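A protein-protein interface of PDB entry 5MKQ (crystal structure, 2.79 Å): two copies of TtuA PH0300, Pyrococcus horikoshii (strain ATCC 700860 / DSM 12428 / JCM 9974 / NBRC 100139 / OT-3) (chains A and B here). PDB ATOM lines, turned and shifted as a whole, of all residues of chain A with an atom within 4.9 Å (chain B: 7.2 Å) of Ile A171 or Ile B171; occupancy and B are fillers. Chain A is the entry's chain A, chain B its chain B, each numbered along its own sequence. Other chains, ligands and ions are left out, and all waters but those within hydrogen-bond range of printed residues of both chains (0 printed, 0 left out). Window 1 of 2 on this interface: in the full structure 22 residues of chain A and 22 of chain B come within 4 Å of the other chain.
The backbone carbonyl oxygen of Phe A252 sits at hydrogen-bond distance from the indole nitrogen of Trp B174.
NE1 of Trp A174 sits close to N of Tyr B256 (3.4 Å).
The indole nitrogen of Trp A174 is in hydrogen-bond range of the backbone carbonyl oxygen of Phe B252 (3.0 Å).
The backbone carbonyl oxygen (O) of Leu B179 is in hydrogen-bond range of the side-chain hydroxyl (OH) of Tyr B256, at 2.6 Å.
The backbone carbonyl oxygen of Asn A169 is in hydrogen-bond range of a ring nitrogen (ND1) of His A173 (3.0 Å).
The indole nitrogen (NE1) of Trp A174 lies close to the backbone carbonyl oxygen (O) of Ile A171, at 3.2 Å.
The backbone carbonyl oxygen of Ile B171 lies close to the indole nitrogen of Trp B174, 3.2 Å away.
Leu B168 touches Leu A168.
CG2 of Ile B171 touches CG2 of Ile A171, 3.8 Å away.
Ile A171 touches Trp B174.
Phe B252 touches Ile A171.
Leu A172 touches Phe B252.
His A173 touches Asn B251.
Trp A174 touches Gly B255.
Trp A174 touches Phe B263.
Phe A252 touches Ile B171 (CE1 to CG2, 3.7 Å).
O of Leu B172 touches CA of Phe A252, at 3.6 Å.
Of chain B, only Ile B171 (3.8 Å), Trp B174 (3.8 Å) and Phe B252 (3.8 Å) come within 4 Å of Ile A171.
Of the printed residues of chain A, Ile B171 touches Ile A171 (3.8 Å), Trp A174 (3.9 Å) and Phe A252 (3.7 Å).
Of the printed residues of chain B, His A173 touches Asn B251.
Of the printed residues of chain A, Asn B251 touches His A173 (3.9 Å).
Of the printed residues of chain B, Leu A172 touches Phe B252 (3.6 Å).
Thr B176 touches none of the printed residues of chain A.
The nearest residue of chain B that does not touch Ile A171 is Leu B168 (6.2 Å).
The nearest printed residue of chain A that does not touch Ile B171 is Leu A168 (6.0 Å).
The nearest printed residue of chain A that does not touch Trp B174 is Leu A167 (5.2 Å).
Of the 19 printed residues of chain B, 9 touch a printed residue of chain A.
Hydrophobic or aromatic side chains of chain B within 4 Å of the printed part of chain A: Leu B168, Ile B171, Leu B172, Trp B174, Phe B252, Tyr B256 and Phe B263.
Among the printed residues, 14 pairs touch across the chains.
Among the printed residues, no Asp or Glu carboxylate lies within 4 Å of a Lys or Arg side-chain nitrogen of the other chain.
Leu B168 touches its own counterpart, Leu A168.
Ile B171 touches its own counterpart, Ile A171.
Leu A172 touches Phe B252, and with the chains exchanged Phe A252 touches Leu B172.
Trp A174 touches Phe B252, and with the chains exchanged Phe A252 touches Trp B174.
Positions printed for both chains: 167, 168, 169, 170, 171, 172, 173, 174, 179 and 252.
Of the 14 pairs that touch across the chains among the printed residues, 10 have their exchanged pair printed and touching as well.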
ATOM      1  N   LEU A 167      -3.334  29.264  19.020  1.00  0.00           N
ATOM      2  CA  LEU A 167      -4.051  29.052  17.761  1.00  0.00           C
ATOM      3  C   LEU A 167      -5.051  27.919  17.882  1.00  0.00           C
ATOM      4  O   LEU A 167      -6.217  28.098  17.531  1.00  0.00           O
ATOM      5  CB  LEU A 167      -3.085  28.735  16.607  1.00  0.00           C
ATOM      6  CG  LEU A 167      -2.233  29.856  16.038  1.00  0.00           C
ATOM      7  CD1 LEU A 167      -1.433  29.356  14.852  1.00  0.00           C
ATOM      8  CD2 LEU A 167      -3.077  31.072  15.647  1.00  0.00           C
ATOM      9  N   LEU A 168      -4.590  26.754  18.378  1.00  0.00           N
ATOM     10  CA  LEU A 168      -5.414  25.569  18.546  1.00  0.00           C
ATOM     11  C   LEU A 168      -6.623  25.841  19.431  1.00  0.00           C
ATOM     12  O   LEU A 168      -7.730  25.454  19.059  1.00  0.00           O
ATOM     13  CB  LEU A 168      -4.577  24.389  19.071  1.00  0.00           C
ATOM     14  CG  LEU A 168      -5.290  23.022  19.176  1.00  0.00           C
ATOM     15  CD1 LEU A 168      -5.722  22.500  17.819  1.00  0.00           C
ATOM     16  CD2 LEU A 168      -4.410  22.004  19.856  1.00  0.00           C
ATOM     17  N   ASN A 169      -6.424  26.536  20.570  1.00  0.00           N
ATOM     18  CA  ASN A 169      -7.511  26.858  21.495  1.00  0.00           C
ATOM     19  C   ASN A 169      -8.526  27.773  20.846  1.00  0.00           C
ATOM     20  O   ASN A 169      -9.720  27.484  20.905  1.00  0.00           O
ATOM     21  CB  ASN A 169      -6.988  27.467  22.802  1.00  0.00           C
ATOM     22  CG  ASN A 169      -8.073  27.744  23.821  1.00  0.00           C
ATOM     23  OD1 ASN A 169      -8.673  28.829  23.855  1.00  0.00           O
ATOM     24  ND2 ASN A 169      -8.367  26.762  24.657  1.00  0.00           N
ATOM     25  N   ASN A 170      -8.048  28.852  20.206  1.00  0.00           N
ATOM     26  CA  ASN A 170      -8.879  29.859  19.547  1.00  0.00           C
ATOM     27  C   ASN A 170      -9.648  29.327  18.347  1.00  0.00           C
ATOM     28  O   ASN A 170     -10.775  29.761  18.130  1.00  0.00           O
ATOM     29  CB  ASN A 170      -8.069  31.089  19.198  1.00  0.00           C
ATOM     30  CG  ASN A 170      -7.902  31.966  20.405  1.00  0.00           C
ATOM     31  OD1 ASN A 170      -8.759  32.791  20.711  1.00  0.00           O
ATOM     32  ND2 ASN A 170      -6.872  31.724  21.192  1.00  0.00           N
ATOM     33  N   ILE A 171      -9.073  28.363  17.607  1.00  0.00           N
ATOM     34  CA  ILE A 171      -9.745  27.706  16.482  1.00  0.00           C
ATOM     35  C   ILE A 171     -10.878  26.818  17.020  1.00  0.00           C
ATOM     36  O   ILE A 171     -11.993  26.897  16.507  1.00  0.00           O
ATOM     37  CB  ILE A 171      -8.728  26.975  15.554  1.00  0.00           C
ATOM     38  CG1 ILE A 171      -8.191  27.954  14.490  1.00  0.00           C
ATOM     39  CG2 ILE A 171      -9.328  25.722  14.888  1.00  0.00           C
ATOM     40  CD1 ILE A 171      -6.742  27.835  14.194  1.00  0.00           C
ATOM     41  N   LEU A 172     -10.608  26.036  18.087  1.00  0.00           N
ATOM     42  CA  LEU A 172     -11.596  25.181  18.741  1.00  0.00           C
ATOM     43  C   LEU A 172     -12.812  25.967  19.246  1.00  0.00           C
ATOM     44  O   LEU A 172     -13.935  25.477  19.127  1.00  0.00           O
ATOM     45  CB  LEU A 172     -10.970  24.369  19.883  1.00  0.00           C
ATOM     46  CG  LEU A 172     -10.109  23.170  19.483  1.00  0.00           C
ATOM     47  CD1 LEU A 172      -9.266  22.727  20.623  1.00  0.00           C
ATOM     48  CD2 LEU A 172     -10.949  22.007  19.005  1.00  0.00           C
ATOM     49  N   HIS A 173     -12.593  27.188  19.779  1.00  0.00           N
ATOM     50  CA  HIS A 173     -13.657  28.067  20.274  1.00  0.00           C
ATOM     51  C   HIS A 173     -14.095  29.091  19.229  1.00  0.00           C
ATOM     52  O   HIS A 173     -14.974  29.910  19.509  1.00  0.00           O
ATOM     53  CB  HIS A 173     -13.227  28.772  21.566  1.00  0.00           C
ATOM     54  CG  HIS A 173     -13.001  27.829  22.699  1.00  0.00           C
ATOM     55  ND1 HIS A 173     -11.728  27.532  23.143  1.00  0.00           N
ATOM     56  CD2 HIS A 173     -13.895  27.116  23.418  1.00  0.00           C
ATOM     57  CE1 HIS A 173     -11.886  26.656  24.120  1.00  0.00           C
ATOM     58  NE2 HIS A 173     -13.172  26.376  24.322  1.00  0.00           N
ATOM     59  N   TRP A 174     -13.488  29.036  18.024  1.00  0.00           N
ATOM     60  CA  TRP A 174     -13.747  29.916  16.880  1.00  0.00           C
ATOM     61  C   TRP A 174     -13.796  31.406  17.278  1.00  0.00           C
ATOM     62  O   TRP A 174     -14.779  32.103  17.000  1.00  0.00           O
ATOM     63  CB  TRP A 174     -14.983  29.462  16.086  1.00  0.00           C
ATOM     64  CG  TRP A 174     -14.724  28.202  15.311  1.00  0.00           C
ATOM     65  CD1 TRP A 174     -15.005  26.923  15.699  1.00  0.00           C
ATOM     66  CD2 TRP A 174     -14.025  28.100  14.064  1.00  0.00           C
ATOM     67  NE1 TRP A 174     -14.547  26.031  14.757  1.00  0.00           N
ATOM     68  CE2 TRP A 174     -13.945  26.726  13.740  1.00  0.00           C
ATOM     69  CE3 TRP A 174     -13.466  29.040  13.180  1.00  0.00           C
ATOM     70  CZ2 TRP A 174     -13.343  26.271  12.563  1.00  0.00           C
ATOM     71  CZ3 TRP A 174     -12.870  28.586  12.015  1.00  0.00           C
ATOM     72  CH2 TRP A 174     -12.813  27.219  11.714  1.00  0.00           C
ATOM     73  N   LEU A 179      -7.898  35.543  16.453  1.00  0.00           N
ATOM     74  CA  LEU A 179      -7.158  34.947  15.336  1.00  0.00           C
ATOM     75  C   LEU A 179      -6.805  36.006  14.300  1.00  0.00           C
ATOM     76  O   LEU A 179      -5.837  35.834  13.564  1.00  0.00           O
ATOM     77  CB  LEU A 179      -7.975  33.824  14.666  1.00  0.00           C
ATOM     78  CG  LEU A 179      -8.201  32.539  15.455  1.00  0.00           C
ATOM     79  CD1 LEU A 179      -9.305  31.720  14.823  1.00  0.00           C
ATOM     80  CD2 LEU A 179      -6.921  31.720  15.572  1.00  0.00           C
ATOM     81  N   PHE A 252       1.847  24.672  10.751  1.00  0.00           N
ATOM     82  CA  PHE A 252       0.557  25.171  11.231  1.00  0.00           C
ATOM     83  C   PHE A 252       0.628  26.668  11.527  1.00  0.00           C
ATOM     84  O   PHE A 252      -0.265  27.409  11.119  1.00  0.00           O
ATOM     85  CB  PHE A 252       0.102  24.367  12.472  1.00  0.00           C
ATOM     86  CG  PHE A 252      -1.147  24.814  13.199  1.00  0.00           C
ATOM     87  CD1 PHE A 252      -2.317  25.096  12.502  1.00  0.00           C
ATOM     88  CD2 PHE A 252      -1.180  24.868  14.586  1.00  0.00           C
ATOM     89  CE1 PHE A 252      -3.473  25.495  13.178  1.00  0.00           C
ATOM     90  CE2 PHE A 252      -2.339  25.255  15.260  1.00  0.00           C
ATOM     91  CZ  PHE A 252      -3.477  25.567  14.551  1.00  0.00           C
ATOM     92  N   ALA B 164     -15.038  16.350  12.778  1.00  0.00           N
ATOM     93  CA  ALA B 164     -14.100  17.009  13.695  1.00  0.00           C
ATOM     94  C   ALA B 164     -12.640  16.731  13.304  1.00  0.00           C
ATOM     95  O   ALA B 164     -11.837  17.662  13.276  1.00  0.00           O
ATOM     96  CB  ALA B 164     -14.370  16.572  15.132  1.00  0.00           C
ATOM     97  N   SER B 165     -12.317  15.458  12.970  1.00  0.00           N
ATOM     98  CA  SER B 165     -10.988  15.015  12.540  1.00  0.00           C
ATOM     99  C   SER B 165     -10.658  15.569  11.164  1.00  0.00           C
ATOM    100  O   SER B 165      -9.495  15.879  10.895  1.00  0.00           O
ATOM    101  CB  SER B 165     -10.890  13.494  12.545  1.00  0.00           C
ATOM    102  OG  SER B 165     -11.847  12.907  11.682  1.00  0.00           O
ATOM    103  N   PHE B 166     -11.681  15.714  10.300  1.00  0.00           N
ATOM    104  CA  PHE B 166     -11.528  16.297   8.973  1.00  0.00           C
ATOM    105  C   PHE B 166     -11.172  17.772   9.156  1.00  0.00           C
ATOM    106  O   PHE B 166     -10.228  18.239   8.525  1.00  0.00           O
ATOM    107  CB  PHE B 166     -12.812  16.115   8.140  1.00  0.00           C
ATOM    108  CG  PHE B 166     -13.068  17.178   7.096  1.00  0.00           C
ATOM    109  CD1 PHE B 166     -12.445  17.119   5.852  1.00  0.00           C
ATOM    110  CD2 PHE B 166     -13.935  18.240   7.355  1.00  0.00           C
ATOM    111  CE1 PHE B 166     -12.667  18.116   4.893  1.00  0.00           C
ATOM    112  CE2 PHE B 166     -14.152  19.240   6.399  1.00  0.00           C
ATOM    113  CZ  PHE B 166     -13.522  19.167   5.172  1.00  0.00           C
ATOM    114  N   LEU B 167     -11.905  18.485  10.048  1.00  0.00           N
ATOM    115  CA  LEU B 167     -11.689  19.902  10.359  1.00  0.00           C
ATOM    116  C   LEU B 167     -10.314  20.130  10.951  1.00  0.00           C
ATOM    117  O   LEU B 167      -9.588  21.001  10.473  1.00  0.00           O
ATOM    118  CB  LEU B 167     -12.745  20.434  11.344  1.00  0.00           C
ATOM    119  CG  LEU B 167     -14.164  20.671  10.843  1.00  0.00           C
ATOM    120  CD1 LEU B 167     -15.010  21.285  11.946  1.00  0.00           C
ATOM    121  CD2 LEU B 167     -14.189  21.549   9.596  1.00  0.00           C
ATOM    122  N   LEU B 168      -9.961  19.347  11.988  1.00  0.00           N
ATOM    123  CA  LEU B 168      -8.688  19.441  12.678  1.00  0.00           C
ATOM    124  C   LEU B 168      -7.513  19.258  11.726  1.00  0.00           C
ATOM    125  O   LEU B 168      -6.573  20.056  11.777  1.00  0.00           O
ATOM    126  CB  LEU B 168      -8.621  18.451  13.854  1.00  0.00           C
ATOM    127  CG  LEU B 168      -7.384  18.534  14.759  1.00  0.00           C
ATOM    128  CD1 LEU B 168      -7.292  19.882  15.479  1.00  0.00           C
ATOM    129  CD2 LEU B 168      -7.373  17.403  15.761  1.00  0.00           C
ATOM    130  N   ASN B 169      -7.580  18.243  10.838  1.00  0.00           N
ATOM    131  CA  ASN B 169      -6.512  17.977   9.873  1.00  0.00           C
ATOM    132  C   ASN B 169      -6.351  19.129   8.904  1.00  0.00           C
ATOM    133  O   ASN B 169      -5.231  19.601   8.710  1.00  0.00           O
ATOM    134  CB  ASN B 169      -6.741  16.656   9.119  1.00  0.00           C
ATOM    135  CG  ASN B 169      -5.609  16.302   8.174  1.00  0.00           C
ATOM    136  OD1 ASN B 169      -5.606  16.683   6.994  1.00  0.00           O
ATOM    137  ND2 ASN B 169      -4.606  15.590   8.680  1.00  0.00           N
ATOM    138  N   ASN B 170      -7.473  19.594   8.324  1.00  0.00           N
ATOM    139  CA  ASN B 170      -7.512  20.674   7.342  1.00  0.00           C
ATOM    140  C   ASN B 170      -7.086  22.021   7.896  1.00  0.00           C
ATOM    141  O   ASN B 170      -6.458  22.782   7.171  1.00  0.00           O
ATOM    142  CB  ASN B 170      -8.866  20.742   6.669  1.00  0.00           C
ATOM    143  CG  ASN B 170      -8.965  19.704   5.585  1.00  0.00           C
ATOM    144  OD1 ASN B 170      -8.549  19.929   4.451  1.00  0.00           O
ATOM    145  ND2 ASN B 170      -9.390  18.503   5.933  1.00  0.00           N
ATOM    146  N   ILE B 171      -7.377  22.298   9.177  1.00  0.00           N
ATOM    147  CA  ILE B 171      -6.944  23.522   9.862  1.00  0.00           C
ATOM    148  C   ILE B 171      -5.421  23.478  10.065  1.00  0.00           C
ATOM    149  O   ILE B 171      -4.747  24.455   9.747  1.00  0.00           O
ATOM    150  CB  ILE B 171      -7.763  23.775  11.161  1.00  0.00           C
ATOM    151  CG1 ILE B 171      -9.036  24.569  10.823  1.00  0.00           C
ATOM    152  CG2 ILE B 171      -6.940  24.495  12.244  1.00  0.00           C
ATOM    153  CD1 ILE B 171     -10.251  24.140  11.547  1.00  0.00           C
ATOM    154  N   LEU B 172      -4.883  22.328  10.523  1.00  0.00           N
ATOM    155  CA  LEU B 172      -3.448  22.119  10.714  1.00  0.00           C
ATOM    156  C   LEU B 172      -2.649  22.334   9.425  1.00  0.00           C
ATOM    157  O   LEU B 172      -1.566  22.908   9.483  1.00  0.00           O
ATOM    158  CB  LEU B 172      -3.158  20.728  11.301  1.00  0.00           C
ATOM    159  CG  LEU B 172      -3.443  20.531  12.787  1.00  0.00           C
ATOM    160  CD1 LEU B 172      -3.497  19.081  13.125  1.00  0.00           C
ATOM    161  CD2 LEU B 172      -2.403  21.216  13.656  1.00  0.00           C
ATOM    162  N   HIS B 173      -3.194  21.901   8.265  1.00  0.00           N
ATOM    163  CA  HIS B 173      -2.565  22.059   6.946  1.00  0.00           C
ATOM    164  C   HIS B 173      -3.071  23.291   6.209  1.00  0.00           C
ATOM    165  O   HIS B 173      -2.641  23.540   5.083  1.00  0.00           O
ATOM    166  CB  HIS B 173      -2.761  20.799   6.091  1.00  0.00           C
ATOM    167  CG  HIS B 173      -2.084  19.598   6.661  1.00  0.00           C
ATOM    168  ND1 HIS B 173      -2.807  18.582   7.263  1.00  0.00           N
ATOM    169  CD2 HIS B 173      -0.764  19.310   6.750  1.00  0.00           C
ATOM    170  CE1 HIS B 173      -1.910  17.704   7.684  1.00  0.00           C
ATOM    171  NE2 HIS B 173      -0.666  18.100   7.399  1.00  0.00           N
ATOM    172  N   TRP B 174      -3.977  24.062   6.850  1.00  0.00           N
ATOM    173  CA  TRP B 174      -4.599  25.285   6.335  1.00  0.00           C
ATOM    174  C   TRP B 174      -5.106  25.128   4.886  1.00  0.00           C
ATOM    175  O   TRP B 174      -4.738  25.912   3.999  1.00  0.00           O
ATOM    176  CB  TRP B 174      -3.682  26.507   6.521  1.00  0.00           C
ATOM    177  CG  TRP B 174      -3.590  26.926   7.958  1.00  0.00           C
ATOM    178  CD1 TRP B 174      -2.621  26.578   8.854  1.00  0.00           C
ATOM    179  CD2 TRP B 174      -4.564  27.678   8.692  1.00  0.00           C
ATOM    180  NE1 TRP B 174      -2.916  27.094  10.094  1.00  0.00           N
ATOM    181  CE2 TRP B 174      -4.103  27.776  10.024  1.00  0.00           C
ATOM    182  CE3 TRP B 174      -5.776  28.304   8.346  1.00  0.00           C
ATOM    183  CZ2 TRP B 174      -4.812  28.467  11.013  1.00  0.00           C
ATOM    184  CZ3 TRP B 174      -6.474  28.993   9.324  1.00  0.00           C
ATOM    185  CH2 TRP B 174      -5.995  29.069  10.642  1.00  0.00           C
ATOM    186  N   ASN B 175      -5.940  24.084   4.663  1.00  0.00           N
ATOM    187  CA  ASN B 175      -6.581  23.774   3.382  1.00  0.00           C
ATOM    188  C   ASN B 175      -7.905  24.526   3.397  1.00  0.00           C
ATOM    189  O   ASN B 175      -8.961  23.945   3.674  1.00  0.00           O
ATOM    190  CB  ASN B 175      -6.832  22.258   3.217  1.00  0.00           C
ATOM    191  CG  ASN B 175      -5.626  21.354   3.320  1.00  0.00           C
ATOM    192  OD1 ASN B 175      -4.569  21.603   2.725  1.00  0.00           O
ATOM    193  ND2 ASN B 175      -5.790  20.238   4.025  1.00  0.00           N
ATOM    194  N   THR B 176      -7.826  25.836   3.149  1.00  0.00           N
ATOM    195  CA  THR B 176      -8.950  26.774   3.183  1.00  0.00           C
ATOM    196  C   THR B 176     -10.051  26.450   2.178  1.00  0.00           C
ATOM    197  O   THR B 176     -11.225  26.656   2.482  1.00  0.00           O
ATOM    198  CB  THR B 176      -8.439  28.199   3.038  1.00  0.00           C
ATOM    199  OG1 THR B 176      -7.556  28.268   1.915  1.00  0.00           O
ATOM    200  CG2 THR B 176      -7.738  28.689   4.296  1.00  0.00           C
ATOM    201  N   LEU B 179     -12.087  23.586   3.670  1.00  0.00           N
ATOM    202  CA  LEU B 179     -12.814  24.162   4.807  1.00  0.00           C
ATOM    203  C   LEU B 179     -13.970  25.030   4.322  1.00  0.00           C
ATOM    204  O   LEU B 179     -14.943  25.209   5.052  1.00  0.00           O
ATOM    205  CB  LEU B 179     -11.877  25.003   5.700  1.00  0.00           C
ATOM    206  CG  LEU B 179     -10.808  24.268   6.499  1.00  0.00           C
ATOM    207  CD1 LEU B 179      -9.770  25.235   7.010  1.00  0.00           C
ATOM    208  CD2 LEU B 179     -11.416  23.475   7.649  1.00  0.00           C
ATOM    209  N   ASN B 251     -19.179  21.769  19.953  1.00  0.00           N
ATOM    210  CA  ASN B 251     -18.938  23.216  19.997  1.00  0.00           C
ATOM    211  C   ASN B 251     -17.970  23.678  18.882  1.00  0.00           C
ATOM    212  O   ASN B 251     -18.148  24.764  18.327  1.00  0.00           O
ATOM    213  CB  ASN B 251     -18.421  23.611  21.385  1.00  0.00           C
ATOM    214  CG  ASN B 251     -18.316  25.096  21.642  1.00  0.00           C
ATOM    215  OD1 ASN B 251     -19.251  25.871  21.403  1.00  0.00           O
ATOM    216  ND2 ASN B 251     -17.189  25.513  22.201  1.00  0.00           N
ATOM    217  N   PHE B 252     -16.978  22.831  18.540  1.00  0.00           N
ATOM    218  CA  PHE B 252     -15.996  23.071  17.481  1.00  0.00           C
ATOM    219  C   PHE B 252     -16.646  22.950  16.097  1.00  0.00           C
ATOM    220  O   PHE B 252     -16.425  23.807  15.246  1.00  0.00           O
ATOM    221  CB  PHE B 252     -14.800  22.102  17.634  1.00  0.00           C
ATOM    222  CG  PHE B 252     -13.738  22.088  16.552  1.00  0.00           C
ATOM    223  CD1 PHE B 252     -13.189  23.273  16.074  1.00  0.00           C
ATOM    224  CD2 PHE B 252     -13.235  20.887  16.064  1.00  0.00           C
ATOM    225  CE1 PHE B 252     -12.200  23.258  15.088  1.00  0.00           C
ATOM    226  CE2 PHE B 252     -12.238  20.872  15.086  1.00  0.00           C
ATOM    227  CZ  PHE B 252     -11.724  22.056  14.608  1.00  0.00           C
ATOM    228  N   GLY B 255     -19.464  25.659  15.751  1.00  0.00           N
ATOM    229  CA  GLY B 255     -18.761  26.929  15.666  1.00  0.00           C
ATOM    230  C   GLY B 255     -18.203  27.139  14.279  1.00  0.00           C
ATOM    231  O   GLY B 255     -18.239  28.255  13.754  1.00  0.00           O
ATOM    232  N   TYR B 256     -17.724  26.045  13.663  1.00  0.00           N
ATOM    233  CA  TYR B 256     -17.183  26.042  12.306  1.00  0.00           C
ATOM    234  C   TYR B 256     -18.248  26.438  11.288  1.00  0.00           C
ATOM    235  O   TYR B 256     -17.943  27.208  10.384  1.00  0.00           O
ATOM    236  CB  TYR B 256     -16.554  24.675  11.966  1.00  0.00           C
ATOM    237  CG  TYR B 256     -16.507  24.355  10.486  1.00  0.00           C
ATOM    238  CD1 TYR B 256     -15.619  25.011   9.637  1.00  0.00           C
ATOM    239  CD2 TYR B 256     -17.357  23.403   9.933  1.00  0.00           C
ATOM    240  CE1 TYR B 256     -15.594  24.741   8.270  1.00  0.00           C
ATOM    241  CE2 TYR B 256     -17.335  23.119   8.569  1.00  0.00           C
ATOM    242  CZ  TYR B 256     -16.445  23.785   7.743  1.00  0.00           C
ATOM    243  OH  TYR B 256     -16.415  23.493   6.403  1.00  0.00           O
ATOM    244  N   PHE B 263     -14.084  31.269   4.593  1.00  0.00           N
ATOM    245  CA  PHE B 263     -13.216  30.565   3.651  1.00  0.00           C
ATOM    246  C   PHE B 263     -13.727  30.621   2.206  1.00  0.00           C
ATOM    247  O   PHE B 263     -13.050  30.116   1.305  1.00  0.00           O
ATOM    248  CB  PHE B 263     -12.952  29.121   4.113  1.00  0.00           C
ATOM    249  CG  PHE B 263     -12.597  28.974   5.573  1.00  0.00           C
ATOM    250  CD1 PHE B 263     -11.371  29.423   6.058  1.00  0.00           C
ATOM    251  CD2 PHE B 263     -13.483  28.381   6.463  1.00  0.00           C
ATOM    252  CE1 PHE B 263     -11.046  29.298   7.409  1.00  0.00           C
ATOM    253  CE2 PHE B 263     -13.152  28.242   7.814  1.00  0.00           C
ATOM    254  CZ  PHE B 263     -11.937  28.708   8.279  1.00  0.00           C
